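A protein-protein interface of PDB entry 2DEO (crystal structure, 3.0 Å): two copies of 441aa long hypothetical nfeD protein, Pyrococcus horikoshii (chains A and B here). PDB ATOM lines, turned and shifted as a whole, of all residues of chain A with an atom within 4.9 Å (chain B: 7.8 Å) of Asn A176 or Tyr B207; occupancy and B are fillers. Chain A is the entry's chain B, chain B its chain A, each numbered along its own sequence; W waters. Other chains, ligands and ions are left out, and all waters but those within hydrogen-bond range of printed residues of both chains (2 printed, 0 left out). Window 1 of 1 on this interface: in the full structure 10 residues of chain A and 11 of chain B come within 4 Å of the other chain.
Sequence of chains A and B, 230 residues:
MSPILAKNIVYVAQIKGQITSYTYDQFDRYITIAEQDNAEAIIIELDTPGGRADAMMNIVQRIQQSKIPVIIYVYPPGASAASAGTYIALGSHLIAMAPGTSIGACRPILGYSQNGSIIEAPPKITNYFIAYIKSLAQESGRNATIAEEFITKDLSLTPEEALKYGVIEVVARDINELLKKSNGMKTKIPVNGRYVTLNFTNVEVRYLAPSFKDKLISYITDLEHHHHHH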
ATOM      1  N   ASP A 174     -19.984  -2.590 -14.525  1.00  0.00           N
ATOM      2  CA  ASP A 174     -19.932  -1.174 -14.880  1.00  0.00           C
ATOM      3  C   ASP A 174     -20.468  -0.220 -13.794  1.00  0.00           C
ATOM      4  O   ASP A 174     -20.924  -0.690 -12.757  1.00  0.00           O
ATOM      5  CB  ASP A 174     -20.678  -0.952 -16.164  1.00  0.00           C
ATOM      6  CG  ASP A 174     -22.139  -1.416 -16.107  1.00  0.00           C
ATOM      7  OD1 ASP A 174     -22.700  -1.609 -14.994  1.00  0.00           O
ATOM      8  OD2 ASP A 174     -22.739  -1.560 -17.208  1.00  0.00           O
ATOM      9  N   ILE A 175     -20.468   1.102 -13.980  1.00  0.00           N
ATOM     10  CA  ILE A 175     -20.948   1.913 -12.878  1.00  0.00           C
ATOM     11  C   ILE A 175     -22.277   1.511 -12.368  1.00  0.00           C
ATOM     12  O   ILE A 175     -22.476   1.413 -11.161  1.00  0.00           O
ATOM     13  CB  ILE A 175     -21.030   3.396 -13.189  1.00  0.00           C
ATOM     14  CG1 ILE A 175     -19.624   3.950 -13.294  1.00  0.00           C
ATOM     15  CG2 ILE A 175     -21.713   4.167 -12.056  1.00  0.00           C
ATOM     16  CD1 ILE A 175     -18.835   3.945 -11.929  1.00  0.00           C
ATOM     17  N   ASN A 176     -23.204   1.251 -13.278  1.00  0.00           N
ATOM     18  CA  ASN A 176     -24.549   0.908 -12.880  1.00  0.00           C
ATOM     19  C   ASN A 176     -24.710  -0.363 -12.053  1.00  0.00           C
ATOM     20  O   ASN A 176     -25.468  -0.367 -11.090  1.00  0.00           O
ATOM     21  CB  ASN A 176     -25.442   0.938 -14.107  1.00  0.00           C
ATOM     22  CG  ASN A 176     -26.903   0.915 -13.754  1.00  0.00           C
ATOM     23  OD1 ASN A 176     -27.368   1.568 -12.809  1.00  0.00           O
ATOM     24  ND2 ASN A 176     -27.636   0.149 -14.504  1.00  0.00           N
ATOM     25  N   GLU A 177     -24.012  -1.439 -12.393  1.00  0.00           N
ATOM     26  CA  GLU A 177     -24.091  -2.640 -11.542  1.00  0.00           C
ATOM     27  C   GLU A 177     -23.575  -2.269 -10.191  1.00  0.00           C
ATOM     28  O   GLU A 177     -24.186  -2.594  -9.194  1.00  0.00           O
ATOM     29  CB  GLU A 177     -23.183  -3.739 -12.011  1.00  0.00           C
ATOM     30  CG  GLU A 177     -23.882  -4.792 -12.759  1.00  0.00           C
ATOM     31  CD  GLU A 177     -23.192  -6.155 -12.652  1.00  0.00           C
ATOM     32  OE1 GLU A 177     -22.074  -6.373 -13.218  1.00  0.00           O
ATOM     33  OE2 GLU A 177     -23.798  -7.025 -11.974  1.00  0.00           O
ATOM     34  N   LEU A 178     -22.407  -1.613 -10.171  1.00  0.00           N
ATOM     35  CA  LEU A 178     -21.788  -1.190  -8.934  1.00  0.00           C
ATOM     36  C   LEU A 178     -22.782  -0.486  -8.059  1.00  0.00           C
ATOM     37  O   LEU A 178     -22.856  -0.795  -6.857  1.00  0.00           O
ATOM     38  CB  LEU A 178     -20.606  -0.268  -9.173  1.00  0.00           C
ATOM     39  CG  LEU A 178     -20.123   0.452  -7.893  1.00  0.00           C
ATOM     40  CD1 LEU A 178     -20.225  -0.463  -6.764  1.00  0.00           C
ATOM     41  CD2 LEU A 178     -18.719   0.820  -7.979  1.00  0.00           C
ATOM     42  N   LEU A 179     -23.543   0.454  -8.640  1.00  0.00           N
ATOM     43  CA  LEU A 179     -24.546   1.171  -7.853  1.00  0.00           C
ATOM     44  C   LEU A 179     -25.616   0.210  -7.328  1.00  0.00           C
ATOM     45  O   LEU A 179     -25.892   0.180  -6.142  1.00  0.00           O
ATOM     46  CB  LEU A 179     -25.173   2.267  -8.669  1.00  0.00           C
ATOM     47  CG  LEU A 179     -24.283   3.488  -8.901  1.00  0.00           C
ATOM     48  CD1 LEU A 179     -25.059   4.560  -9.718  1.00  0.00           C
ATOM     49  CD2 LEU A 179     -23.869   4.084  -7.541  1.00  0.00           C
ATOM     50  N   LYS A 180     -26.180  -0.611  -8.189  1.00  0.00           N
ATOM     51  CA  LYS A 180     -27.160  -1.524  -7.729  1.00  0.00           C
ATOM     52  C   LYS A 180     -26.579  -2.426  -6.674  1.00  0.00           C
ATOM     53  O   LYS A 180     -27.218  -2.589  -5.611  1.00  0.00           O
ATOM     54  CB  LYS A 180     -27.704  -2.369  -8.843  1.00  0.00           C
ATOM     55  CG  LYS A 180     -28.435  -1.580  -9.869  1.00  0.00           C
ATOM     56  CD  LYS A 180     -29.396  -2.439 -10.705  1.00  0.00           C
ATOM     57  CE  LYS A 180     -28.720  -3.331 -11.752  1.00  0.00           C
ATOM     58  NZ  LYS A 180     -28.143  -2.595 -12.898  1.00  0.00           N
ATOM     59  N   VAL A 205     -25.683  10.453 -11.567  1.00  0.00           N
ATOM     60  CA  VAL A 205     -24.236  10.288 -11.582  1.00  0.00           C
ATOM     61  C   VAL A 205     -23.593  11.431 -12.345  1.00  0.00           C
ATOM     62  O   VAL A 205     -24.058  11.756 -13.428  1.00  0.00           O
ATOM     63  CB  VAL A 205     -23.839   8.987 -12.273  1.00  0.00           C
ATOM     64  CG1 VAL A 205     -22.338   8.880 -12.365  1.00  0.00           C
ATOM     65  CG2 VAL A 205     -24.370   7.832 -11.534  1.00  0.00           C
ATOM     66  N   TYR A 207     -20.048  12.621 -14.010  1.00  0.00           N
ATOM     67  CA  TYR A 207     -18.702  12.217 -14.418  1.00  0.00           C
ATOM     68  C   TYR A 207     -17.692  13.410 -14.331  1.00  0.00           C
ATOM     69  O   TYR A 207     -17.929  14.434 -14.887  1.00  0.00           O
ATOM     70  CB  TYR A 207     -18.800  11.700 -15.859  1.00  0.00           C
ATOM     71  CG  TYR A 207     -19.409  10.322 -15.934  1.00  0.00           C
ATOM     72  CD1 TYR A 207     -18.622   9.179 -15.676  1.00  0.00           C
ATOM     73  CD2 TYR A 207     -20.807  10.154 -16.090  1.00  0.00           C
ATOM     74  CE1 TYR A 207     -19.225   7.885 -15.559  1.00  0.00           C
ATOM     75  CE2 TYR A 207     -21.429   8.889 -15.959  1.00  0.00           C
ATOM     76  CZ  TYR A 207     -20.642   7.754 -15.699  1.00  0.00           C
ATOM     77  OH  TYR A 207     -21.220   6.505 -15.586  1.00  0.00           O
ATOM     78  N   ILE B   9     -29.715  16.486 -18.278  1.00  0.00           N
ATOM     79  CA  ILE B   9     -29.853  15.076 -17.955  1.00  0.00           C
ATOM     80  C   ILE B   9     -29.746  14.114 -19.109  1.00  0.00           C
ATOM     81  O   ILE B   9     -30.302  14.352 -20.144  1.00  0.00           O
ATOM     82  CB  ILE B   9     -31.206  14.812 -17.368  1.00  0.00           C
ATOM     83  CG1 ILE B   9     -31.364  15.561 -16.054  1.00  0.00           C
ATOM     84  CG2 ILE B   9     -31.396  13.348 -17.178  1.00  0.00           C
ATOM     85  CD1 ILE B   9     -32.837  15.473 -15.473  1.00  0.00           C
ATOM     86  N   VAL B  10     -29.036  13.020 -18.907  1.00  0.00           N
ATOM     87  CA  VAL B  10     -28.997  11.976 -19.882  1.00  0.00           C
ATOM     88  C   VAL B  10     -29.536  10.728 -19.206  1.00  0.00           C
ATOM     89  O   VAL B  10     -29.029  10.368 -18.126  1.00  0.00           O
ATOM     90  CB  VAL B  10     -27.629  11.731 -20.341  1.00  0.00           C
ATOM     91  CG1 VAL B  10     -27.560  10.405 -21.097  1.00  0.00           C
ATOM     92  CG2 VAL B  10     -27.275  12.860 -21.272  1.00  0.00           C
ATOM     93  N   TYR B  11     -30.569  10.099 -19.799  1.00  0.00           N
ATOM     94  CA  TYR B  11     -31.175   8.864 -19.262  1.00  0.00           C
ATOM     95  C   TYR B  11     -30.545   7.637 -19.884  1.00  0.00           C
ATOM     96  O   TYR B  11     -30.194   7.653 -21.060  1.00  0.00           O
ATOM     97  CB  TYR B  11     -32.690   8.846 -19.515  1.00  0.00           C
ATOM     98  CG  TYR B  11     -33.436   9.593 -18.445  1.00  0.00           C
ATOM     99  CD1 TYR B  11     -33.658   9.018 -17.174  1.00  0.00           C
ATOM    100  CD2 TYR B  11     -33.880  10.917 -18.651  1.00  0.00           C
ATOM    101  CE1 TYR B  11     -34.299   9.736 -16.145  1.00  0.00           C
ATOM    102  CE2 TYR B  11     -34.528  11.659 -17.602  1.00  0.00           C
ATOM    103  CZ  TYR B  11     -34.725  11.045 -16.363  1.00  0.00           C
ATOM    104  OH  TYR B  11     -35.355  11.742 -15.340  1.00  0.00           O
ATOM    105  N   VAL B  12     -30.400   6.575 -19.111  1.00  0.00           N
ATOM    106  CA  VAL B  12     -29.825   5.311 -19.618  1.00  0.00           C
ATOM    107  C   VAL B  12     -30.735   4.106 -19.281  1.00  0.00           C
ATOM    108  O   VAL B  12     -31.111   3.932 -18.140  1.00  0.00           O
ATOM    109  CB  VAL B  12     -28.391   5.118 -19.039  1.00  0.00           C
ATOM    110  CG1 VAL B  12     -27.801   3.770 -19.469  1.00  0.00           C
ATOM    111  CG2 VAL B  12     -27.468   6.216 -19.623  1.00  0.00           C
ATOM    112  N   ALA B  13     -31.092   3.282 -20.247  1.00  0.00           N
ATOM    113  CA  ALA B  13     -31.999   2.183 -19.954  1.00  0.00           C
ATOM    114  C   ALA B  13     -31.587   0.992 -20.749  1.00  0.00           C
ATOM    115  O   ALA B  13     -31.074   1.158 -21.868  1.00  0.00           O
ATOM    116  CB  ALA B  13     -33.418   2.556 -20.338  1.00  0.00           C
ATOM    117  N   GLN B  14     -31.836  -0.208 -20.209  1.00  0.00           N
ATOM    118  CA  GLN B  14     -31.472  -1.463 -20.895  1.00  0.00           C
ATOM    119  C   GLN B  14     -32.700  -2.081 -21.549  1.00  0.00           C
ATOM    120  O   GLN B  14     -33.823  -1.751 -21.223  1.00  0.00           O
ATOM    121  CB  GLN B  14     -30.851  -2.480 -19.933  1.00  0.00           C
ATOM    122  N   TYR B  30     -39.623   4.520 -21.020  1.00  0.00           N
ATOM    123  CA  TYR B  30     -38.321   5.149 -20.912  1.00  0.00           C
ATOM    124  C   TYR B  30     -38.241   6.461 -21.717  1.00  0.00           C
ATOM    125  O   TYR B  30     -37.966   7.526 -21.176  1.00  0.00           O
ATOM    126  CB  TYR B  30     -37.284   4.130 -21.424  1.00  0.00           C
ATOM    127  CG  TYR B  30     -37.155   2.816 -20.612  1.00  0.00           C
ATOM    128  CD1 TYR B  30     -36.825   1.601 -21.262  1.00  0.00           C
ATOM    129  CD2 TYR B  30     -37.244   2.822 -19.188  1.00  0.00           C
ATOM    130  CE1 TYR B  30     -36.579   0.435 -20.516  1.00  0.00           C
ATOM    131  CE2 TYR B  30     -36.992   1.679 -18.444  1.00  0.00           C
ATOM    132  CZ  TYR B  30     -36.657   0.492 -19.101  1.00  0.00           C
ATOM    133  OH  TYR B  30     -36.338  -0.621 -18.356  1.00  0.00           O
ATOM    134  N   GLU B  45     -29.393   0.849 -23.774  1.00  0.00           N
ATOM    135  CA  GLU B  45     -28.314  -0.134 -23.935  1.00  0.00           C
ATOM    136  C   GLU B  45     -29.126  -1.281 -24.524  1.00  0.00           C
ATOM    137  O   GLU B  45     -30.078  -1.811 -23.886  1.00  0.00           O
ATOM    138  CB  GLU B  45     -27.660  -0.539 -22.614  1.00  0.00           C
ATOM    139  CG  GLU B  45     -27.294   0.596 -21.746  1.00  0.00           C
ATOM    140  CD  GLU B  45     -26.597   0.100 -20.512  1.00  0.00           C
ATOM    141  OE1 GLU B  45     -26.973  -1.035 -20.118  1.00  0.00           O
ATOM    142  OE2 GLU B  45     -25.691   0.790 -19.914  1.00  0.00           O
ATOM    143  N   TYR B  75     -24.930  -2.519 -26.309  1.00  0.00           N
ATOM    144  CA  TYR B  75     -24.093  -2.846 -25.161  1.00  0.00           C
ATOM    145  C   TYR B  75     -24.824  -3.911 -24.317  1.00  0.00           C
ATOM    146  O   TYR B  75     -26.031  -4.011 -24.353  1.00  0.00           O
ATOM    147  CB  TYR B  75     -23.940  -1.498 -24.417  1.00  0.00           C
ATOM    148  CG  TYR B  75     -23.223  -1.502 -23.085  1.00  0.00           C
ATOM    149  CD1 TYR B  75     -21.904  -1.104 -23.014  1.00  0.00           C
ATOM    150  CD2 TYR B  75     -23.906  -1.771 -21.897  1.00  0.00           C
ATOM    151  CE1 TYR B  75     -21.280  -0.941 -21.829  1.00  0.00           C
ATOM    152  CE2 TYR B  75     -23.298  -1.621 -20.679  1.00  0.00           C
ATOM    153  CZ  TYR B  75     -21.965  -1.183 -20.635  1.00  0.00           C
ATOM    154  OH  TYR B  75     -21.323  -0.842 -19.441  1.00  0.00           O
ATOM    155  N   ASP B 174     -17.844   2.228 -22.526  1.00  0.00           N
ATOM    156  CA  ASP B 174     -18.812   2.401 -21.458  1.00  0.00           C
ATOM    157  C   ASP B 174     -19.679   3.701 -21.563  1.00  0.00           C
ATOM    158  O   ASP B 174     -19.411   4.557 -22.402  1.00  0.00           O
ATOM    159  CB  ASP B 174     -18.044   2.341 -20.135  1.00  0.00           C
ATOM    160  CG  ASP B 174     -17.047   3.535 -19.918  1.00  0.00           C
ATOM    161  OD1 ASP B 174     -17.032   4.549 -20.686  1.00  0.00           O
ATOM    162  OD2 ASP B 174     -16.265   3.464 -18.921  1.00  0.00           O
ATOM    163  N   ILE B 175     -20.722   3.885 -20.760  1.00  0.00           N
ATOM    164  CA  ILE B 175     -21.524   5.098 -20.937  1.00  0.00           C
ATOM    165  C   ILE B 175     -20.675   6.374 -21.032  1.00  0.00           C
ATOM    166  O   ILE B 175     -20.946   7.268 -21.846  1.00  0.00           O
ATOM    167  CB  ILE B 175     -22.514   5.306 -19.756  1.00  0.00           C
ATOM    168  CG1 ILE B 175     -23.586   4.252 -19.802  1.00  0.00           C
ATOM    169  CG2 ILE B 175     -23.104   6.714 -19.758  1.00  0.00           C
ATOM    170  CD1 ILE B 175     -24.409   4.276 -21.052  1.00  0.00           C
ATOM    171  N   ASN B 176     -19.647   6.464 -20.189  1.00  0.00           N
ATOM    172  CA  ASN B 176     -18.814   7.626 -20.152  1.00  0.00           C
ATOM    173  C   ASN B 176     -18.048   7.877 -21.445  1.00  0.00           C
ATOM    174  O   ASN B 176     -18.012   9.005 -21.882  1.00  0.00           O
ATOM    175  CB  ASN B 176     -17.894   7.494 -18.961  1.00  0.00           C
ATOM    176  CG  ASN B 176     -17.240   8.803 -18.563  1.00  0.00           C
ATOM    177  OD1 ASN B 176     -17.810   9.883 -18.785  1.00  0.00           O
ATOM    178  ND2 ASN B 176     -16.042   8.711 -17.948  1.00  0.00           N
ATOM    179  N   LEU B 179     -20.566   9.159 -23.921  1.00  0.00           N
ATOM    180  CA  LEU B 179     -20.878  10.602 -23.829  1.00  0.00           C
ATOM    181  C   LEU B 179     -19.717  11.461 -24.375  1.00  0.00           C
ATOM    182  O   LEU B 179     -19.973  12.350 -25.167  1.00  0.00           O
ATOM    183  CB  LEU B 179     -21.227  11.064 -22.412  1.00  0.00           C
ATOM    184  CG  LEU B 179     -22.475  10.426 -21.878  1.00  0.00           C
ATOM    185  CD1 LEU B 179     -22.631  10.720 -20.401  1.00  0.00           C
ATOM    186  CD2 LEU B 179     -23.649  10.987 -22.651  1.00  0.00           C
ATOM    187  N   GLU B 204     -25.705  15.066 -16.266  1.00  0.00           N
ATOM    188  CA  GLU B 204     -25.912  14.183 -15.133  1.00  0.00           C
ATOM    189  C   GLU B 204     -26.518  12.947 -15.708  1.00  0.00           C
ATOM    190  O   GLU B 204     -27.381  13.064 -16.538  1.00  0.00           O
ATOM    191  CB  GLU B 204     -26.899  14.766 -14.214  1.00  0.00           C
ATOM    192  CG  GLU B 204     -26.336  15.820 -13.437  1.00  0.00           C
ATOM    193  CD  GLU B 204     -27.342  16.257 -12.470  1.00  0.00           C
ATOM    194  OE1 GLU B 204     -26.970  16.974 -11.512  1.00  0.00           O
ATOM    195  OE2 GLU B 204     -28.522  15.863 -12.687  1.00  0.00           O
ATOM    196  N   VAL B 205     -26.095  11.758 -15.314  1.00  0.00           N
ATOM    197  CA  VAL B 205     -26.691  10.566 -15.901  1.00  0.00           C
ATOM    198  C   VAL B 205     -27.673   9.933 -14.914  1.00  0.00           C
ATOM    199  O   VAL B 205     -27.351   9.810 -13.707  1.00  0.00           O
ATOM    200  CB  VAL B 205     -25.609   9.530 -16.270  1.00  0.00           C
ATOM    201  CG1 VAL B 205     -26.244   8.288 -16.863  1.00  0.00           C
ATOM    202  CG2 VAL B 205     -24.657  10.103 -17.293  1.00  0.00           C
ATOM    203  N   ARG B 206     -28.860   9.553 -15.407  1.00  0.00           N
ATOM    204  CA  ARG B 206     -29.826   8.921 -14.547  1.00  0.00           C
ATOM    205  C   ARG B 206     -30.130   7.546 -15.067  1.00  0.00           C
ATOM    206  O   ARG B 206     -30.574   7.402 -16.179  1.00  0.00           O
ATOM    207  CB  ARG B 206     -31.061   9.747 -14.499  1.00  0.00           C
ATOM    208  CG  ARG B 206     -30.778  11.013 -13.825  1.00  0.00           C
ATOM    209  CD  ARG B 206     -32.041  11.648 -13.341  1.00  0.00           C
ATOM    210  NE  ARG B 206     -31.863  13.014 -12.878  1.00  0.00           N
ATOM    211  CZ  ARG B 206     -32.890  13.798 -12.624  1.00  0.00           C
ATOM    212  NH1 ARG B 206     -32.705  15.033 -12.211  1.00  0.00           N
ATOM    213  NH2 ARG B 206     -34.116  13.321 -12.795  1.00  0.00           N
ATOM    214  N   TYR B 207     -29.877   6.522 -14.276  1.00  0.00           N
ATOM    215  CA  TYR B 207     -30.146   5.174 -14.703  1.00  0.00           C
ATOM    216  C   TYR B 207     -31.615   4.757 -14.419  1.00  0.00           C
ATOM    217  O   TYR B 207     -32.113   4.942 -13.331  1.00  0.00           O
ATOM    218  CB  TYR B 207     -29.158   4.268 -13.994  1.00  0.00           C
ATOM    219  CG  TYR B 207     -27.760   4.393 -14.522  1.00  0.00           C
ATOM    220  CD1 TYR B 207     -27.374   3.711 -15.670  1.00  0.00           C
ATOM    221  CD2 TYR B 207     -26.842   5.220 -13.909  1.00  0.00           C
ATOM    222  CE1 TYR B 207     -26.115   3.832 -16.207  1.00  0.00           C
ATOM    223  CE2 TYR B 207     -25.526   5.382 -14.422  1.00  0.00           C
ATOM    224  CZ  TYR B 207     -25.154   4.679 -15.579  1.00  0.00           C
ATOM    225  OH  TYR B 207     -23.834   4.773 -16.094  1.00  0.00           O
ATOM    226  N   LEU B 208     -32.319   4.229 -15.427  1.00  0.00           N
ATOM    227  CA  LEU B 208     -33.723   3.800 -15.323  1.00  0.00           C
ATOM    228  C   LEU B 208     -33.810   2.289 -15.311  1.00  0.00           C
ATOM    229  O   LEU B 208     -33.421   1.646 -16.294  1.00  0.00           O
ATOM    230  CB  LEU B 208     -34.497   4.252 -16.527  1.00  0.00           C
ATOM    231  CG  LEU B 208     -34.605   5.753 -16.728  1.00  0.00           C
ATOM    232  CD1 LEU B 208     -35.458   6.006 -17.991  1.00  0.00           C
ATOM    233  CD2 LEU B 208     -35.240   6.446 -15.556  1.00  0.00           C
ATOM    234  N   ALA B 209     -34.366   1.722 -14.230  1.00  0.00           N
ATOM    235  CA  ALA B 209     -34.520   0.283 -14.092  1.00  0.00           C
ATOM    236  C   ALA B 209     -35.817  -0.279 -14.661  1.00  0.00           C
ATOM    237  O   ALA B 209     -36.870   0.395 -14.710  1.00  0.00           O
ATOM    238  CB  ALA B 209     -34.470  -0.060 -12.712  1.00  0.00           C
ATOM    239  N   PRO B 210     -35.759  -1.535 -15.109  1.00  0.00           N
ATOM    240  CA  PRO B 210     -36.927  -2.194 -15.654  1.00  0.00           C
ATOM    241  C   PRO B 210     -37.919  -2.305 -14.540  1.00  0.00           C
ATOM    242  O   PRO B 210     -37.519  -2.574 -13.408  1.00  0.00           O
ATOM    243  CB  PRO B 210     -36.404  -3.562 -15.998  1.00  0.00           C
ATOM    244  CG  PRO B 210     -35.229  -3.713 -15.098  1.00  0.00           C
ATOM    245  CD  PRO B 210     -34.589  -2.413 -15.191  1.00  0.00           C
HETATM  246  O   HOH W   1     -23.131   2.236 -16.557  1.00  0.00           O
HETATM  247  O   HOH W   2     -19.431   5.012 -17.142  1.00  0.00           O
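Of chain B, only Tyr B207 comes within 4 Å of Asn A176. Of chain A, only Asn A176, Val A205 and Tyr A207 come within 4 Å of Tyr B207. Of the printed residues of chain B, Tyr A207 touches Asn B176, Val B205 and Tyr B207. Printed residues of chain B within 4 Å of Val A205: Glu B204, Val B205 and Tyr B207. Printed residues of chain A within 4 Å of Glu B204: Val A205. Of the printed residues of chain A, Val B205 touches Val A205 and Tyr A207. Printed residues of chain A within 4 Å of Asn B176: Tyr A207 (3.2 Å).
Asn A176 touches Tyr B207, and with the chains exchanged Tyr A207 touches Asn B176. Val A205 touches its own counterpart, Val B205. Val A205 touches Tyr B207, and with the chains exchanged Tyr A207 touches Val B205. Tyr A207 touches its own counterpart, Tyr B207.
Water W1 lies within hydrogen-bond range of OH of Tyr B207 (2.7 Å) and N of Asn A176 (3.4 Å). Water W2 lies within hydrogen-bond range of OH of Tyr A207 (2.8 Å) and N of Asn B176 (3.4 Å).
Hydrophobic or aromatic side chains of chain B within 4 Å of the printed part of chain A: Tyr B75, Val B205 and Tyr B207. Among the printed residues, no Asp or Glu carboxylate lies within 4 Å of a Lys or Arg side-chain nitrogen of the other chain.
The side-chain hydroxyl of Tyr B75 is in hydrogen-bond range of the side-chain carboxylate of Asp A174, 2.7 Å away. The backbone NH (N) of Val B205 sits at hydrogen-bond distance from the backbone carbonyl oxygen (O) of Val A205, at 2.8 Å. OH of Tyr A207 sits at hydrogen-bond distance from OH of Tyr B207 (3.2 Å).
O of Glu B204 lies within hydrogen-bond range of N of Val B10 (2.9 Å). The side-chain carboxylate (OD1) of Asp B174 lies close to the backbone NH (N) of Asn B176, 3.3 Å away. N of Asn A176 sits close to OD1 of Asp A174, 3.4 Å away. N of Glu A177 is in hydrogen-bond range of OD1 of Asp A174 (2.9 Å). The side-chain amide nitrogen of Asn A176 lies close to the side-chain amino group of Lys A180 (3.2 Å).
Among the printed residues, merely in contact across the chains: Tyr A207 with Asn B176, Asn A176 with Tyr B207, Val A205 with Glu B204, Tyr A207 with Val B205 and Val A205 with Tyr B207.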
